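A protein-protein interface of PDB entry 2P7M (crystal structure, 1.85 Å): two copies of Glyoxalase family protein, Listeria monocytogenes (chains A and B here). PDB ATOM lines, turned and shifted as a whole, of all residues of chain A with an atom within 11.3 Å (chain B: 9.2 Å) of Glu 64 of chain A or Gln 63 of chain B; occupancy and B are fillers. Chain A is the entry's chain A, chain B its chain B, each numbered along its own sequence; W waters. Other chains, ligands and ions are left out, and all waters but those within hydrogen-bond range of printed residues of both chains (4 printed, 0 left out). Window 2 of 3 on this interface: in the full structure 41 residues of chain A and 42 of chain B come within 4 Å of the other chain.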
ATOM      1  N   LEU A  10      15.720  13.765 -16.923  1.00  0.00           N
ATOM      2  CA  LEU A  10      15.823  14.088 -18.332  1.00  0.00           C
ATOM      3  C   LEU A  10      16.028  12.793 -19.110  1.00  0.00           C
ATOM      4  O   LEU A  10      16.782  11.916 -18.692  1.00  0.00           O
ATOM      5  CB  LEU A  10      16.999  15.042 -18.580  1.00  0.00           C
ATOM      6  CG  LEU A  10      16.966  16.357 -17.788  1.00  0.00           C
ATOM      7  CD1 LEU A  10      18.177  17.204 -18.133  1.00  0.00           C
ATOM      8  CD2 LEU A  10      15.687  17.111 -18.110  1.00  0.00           C
ATOM      9  N   ILE A  11      15.330  12.671 -20.228  1.00  0.00           N
ATOM     10  CA  ILE A  11      15.443  11.496 -21.078  1.00  0.00           C
ATOM     11  C   ILE A  11      16.324  11.891 -22.261  1.00  0.00           C
ATOM     12  O   ILE A  11      16.107  12.939 -22.873  1.00  0.00           O
ATOM     13  CB  ILE A  11      14.058  11.067 -21.608  1.00  0.00           C
ATOM     14  CG1 ILE A  11      13.086  10.859 -20.439  1.00  0.00           C
ATOM     15  CG2 ILE A  11      14.190   9.796 -22.445  1.00  0.00           C
ATOM     16  CD1 ILE A  11      13.410   9.681 -19.542  1.00  0.00           C
ATOM     17  N   ASP A  60      14.072   6.887 -26.291  1.00  0.00           N
ATOM     18  CA  ASP A  60      13.676   7.463 -27.573  1.00  0.00           C
ATOM     19  C   ASP A  60      12.899   8.772 -27.427  1.00  0.00           C
ATOM     20  O   ASP A  60      13.000   9.659 -28.276  1.00  0.00           O
ATOM     21  CB  ASP A  60      12.822   6.452 -28.346  1.00  0.00           C
ATOM     22  CG  ASP A  60      12.095   7.079 -29.523  1.00  0.00           C
ATOM     23  OD1 ASP A  60      12.770   7.552 -30.461  1.00  0.00           O
ATOM     24  OD2 ASP A  60      10.845   7.103 -29.506  1.00  0.00           O
ATOM     25  N   SER A  61      12.119   8.881 -26.353  1.00  0.00           N
ATOM     26  CA  SER A  61      11.312  10.072 -26.095  1.00  0.00           C
ATOM     27  C   SER A  61      12.054  11.376 -26.377  1.00  0.00           C
ATOM     28  O   SER A  61      13.178  11.581 -25.919  1.00  0.00           O
ATOM     29  CB  SER A  61      10.829  10.078 -24.642  1.00  0.00           C
ATOM     30  OG  SER A  61      10.074   8.915 -24.350  1.00  0.00           O
ATOM     31  N   LEU A  62      11.410  12.252 -27.139  1.00  0.00           N
ATOM     32  CA  LEU A  62      11.983  13.545 -27.478  1.00  0.00           C
ATOM     33  C   LEU A  62      10.910  14.623 -27.413  1.00  0.00           C
ATOM     34  O   LEU A  62       9.993  14.649 -28.234  1.00  0.00           O
ATOM     35  CB  LEU A  62      12.583  13.514 -28.882  1.00  0.00           C
ATOM     36  CG  LEU A  62      13.119  14.855 -29.387  1.00  0.00           C
ATOM     37  CD1 LEU A  62      14.186  15.376 -28.428  1.00  0.00           C
ATOM     38  CD2 LEU A  62      13.691  14.683 -30.789  1.00  0.00           C
ATOM     39  N   GLN A  63      11.027  15.506 -26.432  1.00  0.00           N
ATOM     40  CA  GLN A  63      10.072  16.593 -26.269  1.00  0.00           C
ATOM     41  C   GLN A  63      10.430  17.682 -27.270  1.00  0.00           C
ATOM     42  O   GLN A  63      11.617  17.934 -27.512  1.00  0.00           O
ATOM     43  CB  GLN A  63      10.161  17.164 -24.852  1.00  0.00           C
ATOM     44  CG  GLN A  63       9.058  18.158 -24.500  1.00  0.00           C
ATOM     45  CD  GLN A  63       7.723  17.478 -24.265  1.00  0.00           C
ATOM     46  OE1 GLN A  63       6.836  17.496 -25.123  1.00  0.00           O
ATOM     47  NE2 GLN A  63       7.579  16.857 -23.100  1.00  0.00           N
ATOM     48  N   GLU A  64       9.417  18.322 -27.856  1.00  0.00           N
ATOM     49  CA  GLU A  64       9.674  19.394 -28.811  1.00  0.00           C
ATOM     50  C   GLU A  64      10.283  20.539 -28.014  1.00  0.00           C
ATOM     51  O   GLU A  64      10.021  20.663 -26.816  1.00  0.00           O
ATOM     52  CB  GLU A  64       8.378  19.865 -29.482  1.00  0.00           C
ATOM     53  CG  GLU A  64       7.452  20.693 -28.592  1.00  0.00           C
ATOM     54  CD  GLU A  64       6.562  19.857 -27.687  1.00  0.00           C
ATOM     55  OE1 GLU A  64       6.836  18.653 -27.499  1.00  0.00           O
ATOM     56  OE2 GLU A  64       5.583  20.417 -27.149  1.00  0.00           O
ATOM     57  N   ARG A  65      11.087  21.368 -28.671  1.00  0.00           N
ATOM     58  CA  ARG A  65      11.729  22.498 -28.002  1.00  0.00           C
ATOM     59  C   ARG A  65      10.738  23.553 -27.506  1.00  0.00           C
ATOM     60  O   ARG A  65       9.833  23.958 -28.233  1.00  0.00           O
ATOM     61  CB  ARG A  65      12.739  23.166 -28.936  1.00  0.00           C
ATOM     62  CG  ARG A  65      13.968  22.339 -29.224  1.00  0.00           C
ATOM     63  CD  ARG A  65      15.017  23.166 -29.971  1.00  0.00           C
ATOM     64  NE  ARG A  65      16.295  22.464 -30.029  1.00  0.00           N
ATOM     65  CZ  ARG A  65      17.416  22.971 -30.533  1.00  0.00           C
ATOM     66  NH1 ARG A  65      17.435  24.198 -31.028  1.00  0.00           N
ATOM     67  NH2 ARG A  65      18.518  22.239 -30.543  1.00  0.00           N
ATOM     68  N   THR A  66      10.923  23.995 -26.264  1.00  0.00           N
ATOM     69  CA  THR A  66      10.059  25.013 -25.665  1.00  0.00           C
ATOM     70  C   THR A  66      10.828  25.791 -24.603  1.00  0.00           C
ATOM     71  O   THR A  66      11.982  25.472 -24.303  1.00  0.00           O
ATOM     72  CB  THR A  66       8.800  24.399 -24.991  1.00  0.00           C
ATOM     73  OG1 THR A  66       9.187  23.624 -23.850  1.00  0.00           O
ATOM     74  CG2 THR A  66       8.043  23.512 -25.966  1.00  0.00           C
ATOM     75  N   TYR A  67      10.179  26.803 -24.031  1.00  0.00           N
ATOM     76  CA  TYR A  67      10.815  27.617 -23.011  1.00  0.00           C
ATOM     77  C   TYR A  67      10.664  27.005 -21.619  1.00  0.00           C
ATOM     78  O   TYR A  67      11.079  27.600 -20.623  1.00  0.00           O
ATOM     79  CB  TYR A  67      10.284  29.059 -23.051  1.00  0.00           C
ATOM     80  CG  TYR A  67      11.229  30.061 -22.409  1.00  0.00           C
ATOM     81  CD1 TYR A  67      12.583  30.084 -22.745  1.00  0.00           C
ATOM     82  CD2 TYR A  67      10.775  30.973 -21.456  1.00  0.00           C
ATOM     83  CE1 TYR A  67      13.465  30.993 -22.144  1.00  0.00           C
ATOM     84  CE2 TYR A  67      11.643  31.887 -20.852  1.00  0.00           C
ATOM     85  CZ  TYR A  67      12.986  31.891 -21.200  1.00  0.00           C
ATOM     86  OH  TYR A  67      13.848  32.787 -20.610  1.00  0.00           O
ATOM     87  N   ASN A  68      10.062  25.818 -21.548  1.00  0.00           N
ATOM     88  CA  ASN A  68       9.955  25.111 -20.274  1.00  0.00           C
ATOM     89  C   ASN A  68      11.434  24.787 -20.024  1.00  0.00           C
ATOM     90  O   ASN A  68      12.075  24.171 -20.875  1.00  0.00           O
ATOM     91  CB  ASN A  68       9.169  23.799 -20.432  1.00  0.00           C
ATOM     92  CG  ASN A  68       7.662  24.013 -20.600  1.00  0.00           C
ATOM     93  OD1 ASN A  68       6.934  24.220 -19.625  1.00  0.00           O
ATOM     94  ND2 ASN A  68       7.193  23.960 -21.840  1.00  0.00           N
ATOM     95  N   HIS A  69      11.996  25.201 -18.893  1.00  0.00           N
ATOM     96  CA  HIS A  69      13.414  24.919 -18.673  1.00  0.00           C
ATOM     97  C   HIS A  69      13.888  25.128 -17.246  1.00  0.00           C
ATOM     98  O   HIS A  69      13.170  25.670 -16.408  1.00  0.00           O
ATOM     99  CB  HIS A  69      14.274  25.783 -19.611  1.00  0.00           C
ATOM    100  CG  HIS A  69      14.322  27.235 -19.236  1.00  0.00           C
ATOM    101  ND1 HIS A  69      13.306  28.121 -19.529  1.00  0.00           N
ATOM    102  CD2 HIS A  69      15.271  27.955 -18.590  1.00  0.00           C
ATOM    103  CE1 HIS A  69      13.628  29.322 -19.085  1.00  0.00           C
ATOM    104  NE2 HIS A  69      14.816  29.249 -18.509  1.00  0.00           N
ATOM    105  N   LYS A  94      21.533  30.436 -27.438  1.00  0.00           N
ATOM    106  CA  LYS A  94      20.528  31.397 -27.865  1.00  0.00           C
ATOM    107  C   LYS A  94      21.139  32.788 -27.836  1.00  0.00           C
ATOM    108  O   LYS A  94      22.098  33.035 -27.110  1.00  0.00           O
ATOM    109  CB  LYS A  94      19.336  31.392 -26.908  1.00  0.00           C
ATOM    110  CG  LYS A  94      18.464  30.158 -26.960  1.00  0.00           C
ATOM    111  CD  LYS A  94      17.802  30.022 -28.320  1.00  0.00           C
ATOM    112  CE  LYS A  94      16.565  29.161 -28.224  1.00  0.00           C
ATOM    113  NZ  LYS A  94      16.074  28.754 -29.564  1.00  0.00           N
ATOM    114  N   TYR A 110      21.418  24.538 -25.497  1.00  0.00           N
ATOM    115  CA  TYR A 110      20.789  23.226 -25.518  1.00  0.00           C
ATOM    116  C   TYR A 110      21.755  22.063 -25.312  1.00  0.00           C
ATOM    117  O   TYR A 110      22.970  22.216 -25.456  1.00  0.00           O
ATOM    118  CB  TYR A 110      20.091  22.989 -26.859  1.00  0.00           C
ATOM    119  CG  TYR A 110      18.923  23.894 -27.164  1.00  0.00           C
ATOM    120  CD1 TYR A 110      19.102  25.083 -27.872  1.00  0.00           C
ATOM    121  CD2 TYR A 110      17.626  23.545 -26.770  1.00  0.00           C
ATOM    122  CE1 TYR A 110      18.019  25.904 -28.186  1.00  0.00           C
ATOM    123  CE2 TYR A 110      16.538  24.360 -27.077  1.00  0.00           C
ATOM    124  CZ  TYR A 110      16.741  25.533 -27.784  1.00  0.00           C
ATOM    125  OH  TYR A 110      15.668  26.335 -28.101  1.00  0.00           O
ATOM    126  N   ASP A 111      21.203  20.904 -24.964  1.00  0.00           N
ATOM    127  CA  ASP A 111      22.010  19.700 -24.850  1.00  0.00           C
ATOM    128  C   ASP A 111      21.725  19.014 -26.189  1.00  0.00           C
ATOM    129  O   ASP A 111      21.370  19.693 -27.151  1.00  0.00           O
ATOM    130  CB  ASP A 111      21.598  18.829 -23.651  1.00  0.00           C
ATOM    131  CG  ASP A 111      20.209  18.254 -23.780  1.00  0.00           C
ATOM    132  OD1 ASP A 111      19.892  17.345 -22.980  1.00  0.00           O
ATOM    133  OD2 ASP A 111      19.439  18.700 -24.658  1.00  0.00           O
ATOM    134  N   PHE A 112      21.848  17.696 -26.277  1.00  0.00           N
ATOM    135  CA  PHE A 112      21.619  17.041 -27.566  1.00  0.00           C
ATOM    136  C   PHE A 112      20.231  16.456 -27.687  1.00  0.00           C
ATOM    137  O   PHE A 112      19.947  15.719 -28.633  1.00  0.00           O
ATOM    138  CB  PHE A 112      22.643  15.922 -27.783  1.00  0.00           C
ATOM    139  CG  PHE A 112      24.041  16.288 -27.363  1.00  0.00           C
ATOM    140  CD1 PHE A 112      24.592  15.749 -26.205  1.00  0.00           C
ATOM    141  CD2 PHE A 112      24.800  17.178 -28.116  1.00  0.00           C
ATOM    142  CE1 PHE A 112      25.883  16.089 -25.801  1.00  0.00           C
ATOM    143  CE2 PHE A 112      26.094  17.526 -27.720  1.00  0.00           C
ATOM    144  CZ  PHE A 112      26.635  16.980 -26.559  1.00  0.00           C
ATOM    145  N   ASP A 113      19.361  16.801 -26.739  1.00  0.00           N
ATOM    146  CA  ASP A 113      18.008  16.272 -26.722  1.00  0.00           C
ATOM    147  C   ASP A 113      16.926  17.302 -26.429  1.00  0.00           C
ATOM    148  O   ASP A 113      16.043  17.071 -25.609  1.00  0.00           O
ATOM    149  CB  ASP A 113      17.951  15.134 -25.712  1.00  0.00           C
ATOM    150  CG  ASP A 113      18.879  13.992 -26.089  1.00  0.00           C
ATOM    151  OD1 ASP A 113      18.456  13.129 -26.886  1.00  0.00           O
ATOM    152  OD2 ASP A 113      20.037  13.971 -25.611  1.00  0.00           O
ATOM    153  N   ASN A 114      17.002  18.432 -27.121  1.00  0.00           N
ATOM    154  CA  ASN A 114      16.042  19.517 -26.974  1.00  0.00           C
ATOM    155  C   ASN A 114      15.842  20.067 -25.578  1.00  0.00           C
ATOM    156  O   ASN A 114      14.809  20.663 -25.305  1.00  0.00           O
ATOM    157  CB  ASN A 114      14.680  19.107 -27.522  1.00  0.00           C
ATOM    158  CG  ASN A 114      14.683  18.973 -29.015  1.00  0.00           C
ATOM    159  OD1 ASN A 114      15.583  19.480 -29.691  1.00  0.00           O
ATOM    160  ND2 ASN A 114      13.665  18.304 -29.552  1.00  0.00           N
ATOM    161  N   HIS A 115      16.809  19.876 -24.691  1.00  0.00           N
ATOM    162  CA  HIS A 115      16.668  20.416 -23.345  1.00  0.00           C
ATOM    163  C   HIS A 115      17.342  21.775 -23.271  1.00  0.00           C
ATOM    164  O   HIS A 115      18.559  21.881 -23.436  1.00  0.00           O
ATOM    165  CB  HIS A 115      17.304  19.496 -22.307  1.00  0.00           C
ATOM    166  CG  HIS A 115      16.662  18.149 -22.206  1.00  0.00           C
ATOM    167  ND1 HIS A 115      17.327  16.985 -22.521  1.00  0.00           N
ATOM    168  CD2 HIS A 115      15.429  17.777 -21.786  1.00  0.00           C
ATOM    169  CE1 HIS A 115      16.534  15.952 -22.296  1.00  0.00           C
ATOM    170  NE2 HIS A 115      15.377  16.404 -21.850  1.00  0.00           N
ATOM    171  N   LEU A 116      16.560  22.818 -23.019  1.00  0.00           N
ATOM    172  CA  LEU A 116      17.129  24.151 -22.906  1.00  0.00           C
ATOM    173  C   LEU A 116      17.616  24.383 -21.476  1.00  0.00           C
ATOM    174  O   LEU A 116      16.892  24.118 -20.519  1.00  0.00           O
ATOM    175  CB  LEU A 116      16.081  25.213 -23.234  1.00  0.00           C
ATOM    176  CG  LEU A 116      16.579  26.657 -23.093  1.00  0.00           C
ATOM    177  CD1 LEU A 116      17.558  26.975 -24.213  1.00  0.00           C
ATOM    178  CD2 LEU A 116      15.398  27.615 -23.149  1.00  0.00           C
ATOM    179  N   PHE A 117      18.835  24.879 -21.327  1.00  0.00           N
ATOM    180  CA  PHE A 117      19.351  25.176 -19.996  1.00  0.00           C
ATOM    181  C   PHE A 117      19.627  26.678 -19.909  1.00  0.00           C
ATOM    182  O   PHE A 117      19.974  27.306 -20.910  1.00  0.00           O
ATOM    183  CB  PHE A 117      20.647  24.405 -19.713  1.00  0.00           C
ATOM    184  CG  PHE A 117      20.458  22.925 -19.554  1.00  0.00           C
ATOM    185  CD1 PHE A 117      20.647  22.064 -20.629  1.00  0.00           C
ATOM    186  CD2 PHE A 117      20.107  22.387 -18.320  1.00  0.00           C
ATOM    187  CE1 PHE A 117      20.496  20.683 -20.472  1.00  0.00           C
ATOM    188  CE2 PHE A 117      19.951  21.012 -18.155  1.00  0.00           C
ATOM    189  CZ  PHE A 117      20.148  20.160 -19.236  1.00  0.00           C
ATOM    190  N   ILE B  11       5.686  26.645 -19.066  1.00  0.00           N
ATOM    191  CA  ILE B  11       4.787  27.334 -19.982  1.00  0.00           C
ATOM    192  C   ILE B  11       3.413  26.657 -19.894  1.00  0.00           C
ATOM    193  O   ILE B  11       3.303  25.435 -20.006  1.00  0.00           O
ATOM    194  CB  ILE B  11       5.324  27.271 -21.439  1.00  0.00           C
ATOM    195  CG1 ILE B  11       6.750  27.835 -21.492  1.00  0.00           C
ATOM    196  CG2 ILE B  11       4.413  28.062 -22.381  1.00  0.00           C
ATOM    197  CD1 ILE B  11       6.854  29.280 -21.060  1.00  0.00           C
ATOM    198  N   ASP B  60       1.882  27.964 -25.121  1.00  0.00           N
ATOM    199  CA  ASP B  60       1.382  26.656 -25.540  1.00  0.00           C
ATOM    200  C   ASP B  60       1.719  25.505 -24.592  1.00  0.00           C
ATOM    201  O   ASP B  60       2.788  25.479 -23.975  1.00  0.00           O
ATOM    202  CB  ASP B  60       1.908  26.311 -26.940  1.00  0.00           C
ATOM    203  CG  ASP B  60       1.385  27.245 -28.010  1.00  0.00           C
ATOM    204  OD1 ASP B  60       1.678  27.006 -29.200  1.00  0.00           O
ATOM    205  OD2 ASP B  60       0.686  28.219 -27.670  1.00  0.00           O
ATOM    206  N   SER B  61       0.795  24.554 -24.470  1.00  0.00           N
ATOM    207  CA  SER B  61       1.022  23.387 -23.624  1.00  0.00           C
ATOM    208  C   SER B  61       1.996  22.509 -24.401  1.00  0.00           C
ATOM    209  O   SER B  61       2.197  22.723 -25.594  1.00  0.00           O
ATOM    210  CB  SER B  61      -0.279  22.607 -23.399  1.00  0.00           C
ATOM    211  OG  SER B  61      -1.322  23.444 -22.939  1.00  0.00           O
ATOM    212  N   LEU B  62       2.610  21.539 -23.731  1.00  0.00           N
ATOM    213  CA  LEU B  62       3.529  20.634 -24.414  1.00  0.00           C
ATOM    214  C   LEU B  62       2.654  19.805 -25.361  1.00  0.00           C
ATOM    215  O   LEU B  62       1.539  19.418 -25.004  1.00  0.00           O
ATOM    216  CB  LEU B  62       4.266  19.737 -23.404  1.00  0.00           C
ATOM    217  CG  LEU B  62       5.271  20.455 -22.480  1.00  0.00           C
ATOM    218  CD1 LEU B  62       5.854  19.468 -21.474  1.00  0.00           C
ATOM    219  CD2 LEU B  62       6.388  21.086 -23.314  1.00  0.00           C
ATOM    220  N   GLN B  63       3.157  19.560 -26.569  1.00  0.00           N
ATOM    221  CA  GLN B  63       2.423  18.815 -27.587  1.00  0.00           C
ATOM    222  C   GLN B  63       2.176  17.346 -27.262  1.00  0.00           C
ATOM    223  O   GLN B  63       1.120  16.804 -27.584  1.00  0.00           O
ATOM    224  CB  GLN B  63       3.152  18.929 -28.928  1.00  0.00           C
ATOM    225  CG  GLN B  63       2.995  20.288 -29.597  1.00  0.00           C
ATOM    226  CD  GLN B  63       4.162  20.638 -30.505  1.00  0.00           C
ATOM    227  OE1 GLN B  63       4.627  19.809 -31.290  1.00  0.00           O
ATOM    228  NE2 GLN B  63       4.637  21.877 -30.407  1.00  0.00           N
ATOM    229  N   GLU B  64       3.151  16.708 -26.627  1.00  0.00           N
ATOM    230  CA  GLU B  64       3.038  15.302 -26.265  1.00  0.00           C
ATOM    231  C   GLU B  64       3.597  15.109 -24.866  1.00  0.00           C
ATOM    232  O   GLU B  64       4.338  15.950 -24.366  1.00  0.00           O
ATOM    233  CB  GLU B  64       3.838  14.434 -27.244  1.00  0.00           C
ATOM    234  CG  GLU B  64       3.390  14.509 -28.691  1.00  0.00           C
ATOM    235  CD  GLU B  64       2.146  13.688 -28.974  1.00  0.00           C
ATOM    236  OE1 GLU B  64       1.711  13.662 -30.146  1.00  0.00           O
ATOM    237  OE2 GLU B  64       1.601  13.067 -28.033  1.00  0.00           O
ATOM    238  N   ARG B  65       3.241  13.999 -24.235  1.00  0.00           N
ATOM    239  CA  ARG B  65       3.738  13.707 -22.905  1.00  0.00           C
ATOM    240  C   ARG B  65       5.007  12.874 -23.020  1.00  0.00           C
ATOM    241  O   ARG B  65       5.069  11.945 -23.829  1.00  0.00           O
ATOM    242  CB  ARG B  65       2.687  12.939 -22.109  1.00  0.00           C
ATOM    243  CG  ARG B  65       1.452  13.760 -21.789  1.00  0.00           C
ATOM    244  CD  ARG B  65       0.422  12.939 -21.050  1.00  0.00           C
ATOM    245  NE  ARG B  65      -0.669  13.771 -20.557  1.00  0.00           N
ATOM    246  CZ  ARG B  65      -1.743  13.297 -19.933  1.00  0.00           C
ATOM    247  NH1 ARG B  65      -1.873  11.992 -19.730  1.00  0.00           N
ATOM    248  NH2 ARG B  65      -2.680  14.130 -19.505  1.00  0.00           N
ATOM    249  N   THR B  66       6.017  13.226 -22.225  1.00  0.00           N
ATOM    250  CA  THR B  66       7.285  12.504 -22.208  1.00  0.00           C
ATOM    251  C   THR B  66       7.645  12.230 -20.759  1.00  0.00           C
ATOM    252  O   THR B  66       7.007  12.759 -19.854  1.00  0.00           O
ATOM    253  CB  THR B  66       8.431  13.314 -22.860  1.00  0.00           C
ATOM    254  OG1 THR B  66       8.724  14.476 -22.070  1.00  0.00           O
ATOM    255  CG2 THR B  66       8.045  13.732 -24.267  1.00  0.00           C
ATOM    256  N   ASN B  68      10.261  13.211 -19.239  1.00  0.00           N
ATOM    257  CA  ASN B  68      11.088  14.281 -18.677  1.00  0.00           C
ATOM    258  C   ASN B  68      10.179  14.894 -17.621  1.00  0.00           C
ATOM    259  O   ASN B  68       9.009  15.155 -17.901  1.00  0.00           O
ATOM    260  CB  ASN B  68      11.415  15.336 -19.740  1.00  0.00           C
ATOM    261  CG  ASN B  68      12.384  14.830 -20.796  1.00  0.00           C
ATOM    262  OD1 ASN B  68      13.596  14.738 -20.564  1.00  0.00           O
ATOM    263  ND2 ASN B  68      11.852  14.491 -21.962  1.00  0.00           N
ATOM    264  N   ASP B 113      -1.199  20.848 -18.937  1.00  0.00           N
ATOM    265  CA  ASP B 113      -0.390  21.219 -20.087  1.00  0.00           C
ATOM    266  C   ASP B 113       0.629  20.147 -20.461  1.00  0.00           C
ATOM    267  O   ASP B 113       1.652  20.431 -21.086  1.00  0.00           O
ATOM    268  CB  ASP B 113       0.304  22.554 -19.787  1.00  0.00           C
ATOM    269  CG  ASP B 113      -0.678  23.696 -19.638  1.00  0.00           C
ATOM    270  OD1 ASP B 113      -1.018  24.331 -20.660  1.00  0.00           O
ATOM    271  OD2 ASP B 113      -1.124  23.950 -18.498  1.00  0.00           O
ATOM    272  N   ASN B 114       0.326  18.915 -20.068  1.00  0.00           N
ATOM    273  CA  ASN B 114       1.172  17.765 -20.341  1.00  0.00           C
ATOM    274  C   ASN B 114       2.519  17.771 -19.645  1.00  0.00           C
ATOM    275  O   ASN B 114       3.485  17.243 -20.179  1.00  0.00           O
ATOM    276  CB  ASN B 114       1.370  17.585 -21.852  1.00  0.00           C
ATOM    277  CG  ASN B 114       0.117  17.077 -22.542  1.00  0.00           C
ATOM    278  OD1 ASN B 114      -0.627  16.278 -21.977  1.00  0.00           O
ATOM    279  ND2 ASN B 114      -0.116  17.530 -23.766  1.00  0.00           N
ATOM    280  N   HIS B 115       2.584  18.369 -18.459  1.00  0.00           N
ATOM    281  CA  HIS B 115       3.824  18.372 -17.687  1.00  0.00           C
ATOM    282  C   HIS B 115       3.707  17.217 -16.704  1.00  0.00           C
ATOM    283  O   HIS B 115       2.758  17.157 -15.923  1.00  0.00           O
ATOM    284  CB  HIS B 115       3.995  19.645 -16.852  1.00  0.00           C
ATOM    285  CG  HIS B 115       4.170  20.895 -17.651  1.00  0.00           C
ATOM    286  ND1 HIS B 115       3.304  21.962 -17.548  1.00  0.00           N
ATOM    287  CD2 HIS B 115       5.137  21.276 -18.518  1.00  0.00           C
ATOM    288  CE1 HIS B 115       3.730  22.947 -18.316  1.00  0.00           C
ATOM    289  NE2 HIS B 115       4.840  22.557 -18.916  1.00  0.00           N
HETATM  290  O   HOH W   1       4.303  23.922 -21.994  1.00  0.00           O
HETATM  291  O   HOH W   2       5.653  15.898 -21.308  1.00  0.00           O
HETATM  292  O   HOH W   3      13.777  13.635 -23.810  1.00  0.00           O
HETATM  293  O   HOH W   4       4.493  22.920 -26.946  1.00  0.00           O
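The backbone NH (N) of Ile 11 of chain A is in hydrogen-bond range of the side-chain amide oxygen (OD1) of Asn 68 of chain B, 2.7 Å away. The backbone carbonyl oxygen of Glu 64 of chain B sits close to the side-chain amide oxygen of Gln 63 of chain A (3.0 Å). NE2 of Gln 63 of chain A lies within hydrogen-bond range of OG1 of Thr 66 of chain B (2.8 Å). The side-chain carboxylate (OE2) of Glu 64 of chain A sits at hydrogen-bond distance from the backbone NH (N) of Gln 63 of chain B (2.6 Å). The backbone NH (N) of Ile 11 of chain B is in hydrogen-bond range of the side-chain amide oxygen (OD1) of Asn 68 of chain A (2.8 Å). A ring nitrogen (NE2) of His 115 of chain B sits at hydrogen-bond distance from the side-chain amide oxygen (OD1) of Asn 68 of chain A, at 2.8 Å. A ring nitrogen (NE2) of His 115 of chain A lies within hydrogen-bond range of the side-chain amide oxygen (OD1) of Asn 68 of chain B, 2.8 Å away.
O of Gln 63 of chain A lies within hydrogen-bond range of ND2 of Asn 114 of chain A, at 2.9 Å. OG1 of Thr 66 of chain A is in hydrogen-bond range of ND2 of Asn 68 of chain A (2.9 Å). The side-chain carboxylate (OD1) of Asp 111 of chain A sits at hydrogen-bond distance from a ring nitrogen (ND1) of His 115 of chain A, at 2.6 Å. The backbone carbonyl oxygen (O) of Asp 113 of chain A is in hydrogen-bond range of a ring nitrogen (ND1) of His 115 of chain A (3.3 Å). A ring nitrogen (NE2) of His 115 of chain B sits close to the backbone carbonyl oxygen (O) of Ile 11 of chain B, at 3.4 Å. ND2 of Asn 68 of chain B lies within hydrogen-bond range of OG1 of Thr 66 of chain B (3.1 Å).
CA of Leu 10 of chain A touches OD1 of Asn 68 of chain B (3.2 Å). CD1 of Leu 62 of chain B touches NE2 of Gln 63 of chain A, 3.5 Å away. Glu 64 of chain A touches Leu 62 of chain B. CD2 of Leu 62 of chain B touches OG1 of Thr 66 of chain A, 3.8 Å away. Ile 11 of chain B touches Tyr 67 of chain A. CD2 of Leu 62 of chain B touches ND2 of Asn 68 of chain A (3.3 Å).
Printed residues of chain B within 4 Å of Glu 64 of chain A: Leu 62 (3.4 Å) and Gln 63 (2.6 Å). Printed residues of chain A within 4 Å of Gln 63 of chain B: Glu 64 (2.6 Å). No residue of chain A comes within 4 Å of Ser 61 of chain B. Leu 62 of chain B touches just these residues of chain A: Gln 63, Glu 64, Thr 66 and Asn 68. No residue of chain A comes within 4 Å of Asn 114 of chain B. Of the printed residues of chain A, Thr 66 of chain B touches Gln 63. Of the printed residues of chain B, Ile 11 of chain A touches Asn 68 (2.7 Å). The nearest residue of chain A that does not touch Gln 63 of chain B is Gln 63 of chain A (4.5 Å).
Printed residues of chain B that touch a printed residue of chain A: Ile 11, Leu 62, Gln 63, Glu 64, Thr 66, Asn 68 and His 115. Along chain B the printed residues that touch a printed residue of chain A span positions 11 to 115. Among the printed residues, no Asp or Glu carboxylate lies within 4 Å of a Lys or Arg side-chain nitrogen of the other chain.
Gln 63 of chain A touches Glu 64 of chain B, and with the chains exchanged Glu 64 of chain A touches Gln 63 of chain B. Thr 66 of chain A touches Leu 62 of chain B, but with the chains exchanged Leu 62 of chain A does not touch Thr 66 of chain B (4.3 Å). Asn 68 of chain A touches Leu 62 of chain B, but with the chains exchanged Leu 62 of chain A does not touch Asn 68 of chain B (5.5 Å). Asn 68 of chain A touches His 115 of chain B, and with the chains exchanged His 115 of chain A touches Asn 68 of chain B. 12 positions are printed for both chains.
Water W3 lies within hydrogen-bond range of the backbone carbonyl oxygen (O) of Ile 11 of chain A, the side-chain amide nitrogen (ND2) of Asn 68 of chain B and the backbone carbonyl oxygen (O) of Ser 61 of chain A. Water W4 lies within hydrogen-bond range of the backbone carbonyl oxygen (O) of Ser 61 of chain B and the side-chain carboxylate (OE2) of Glu 64 of chain A. Water W1 lies within hydrogen-bond range of O of Ile 11 of chain B, ND2 of Asn 68 of chain A, O of Asp 60 of chain B, N of Leu 62 of chain B and NE2 of His 115 of chain B. Water W2 lies within hydrogen-bond range of O of Asn 114 of chain B, NE2 of Gln 63 of chain A, N of Thr 66 of chain B and O of Glu 64 of chain B.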
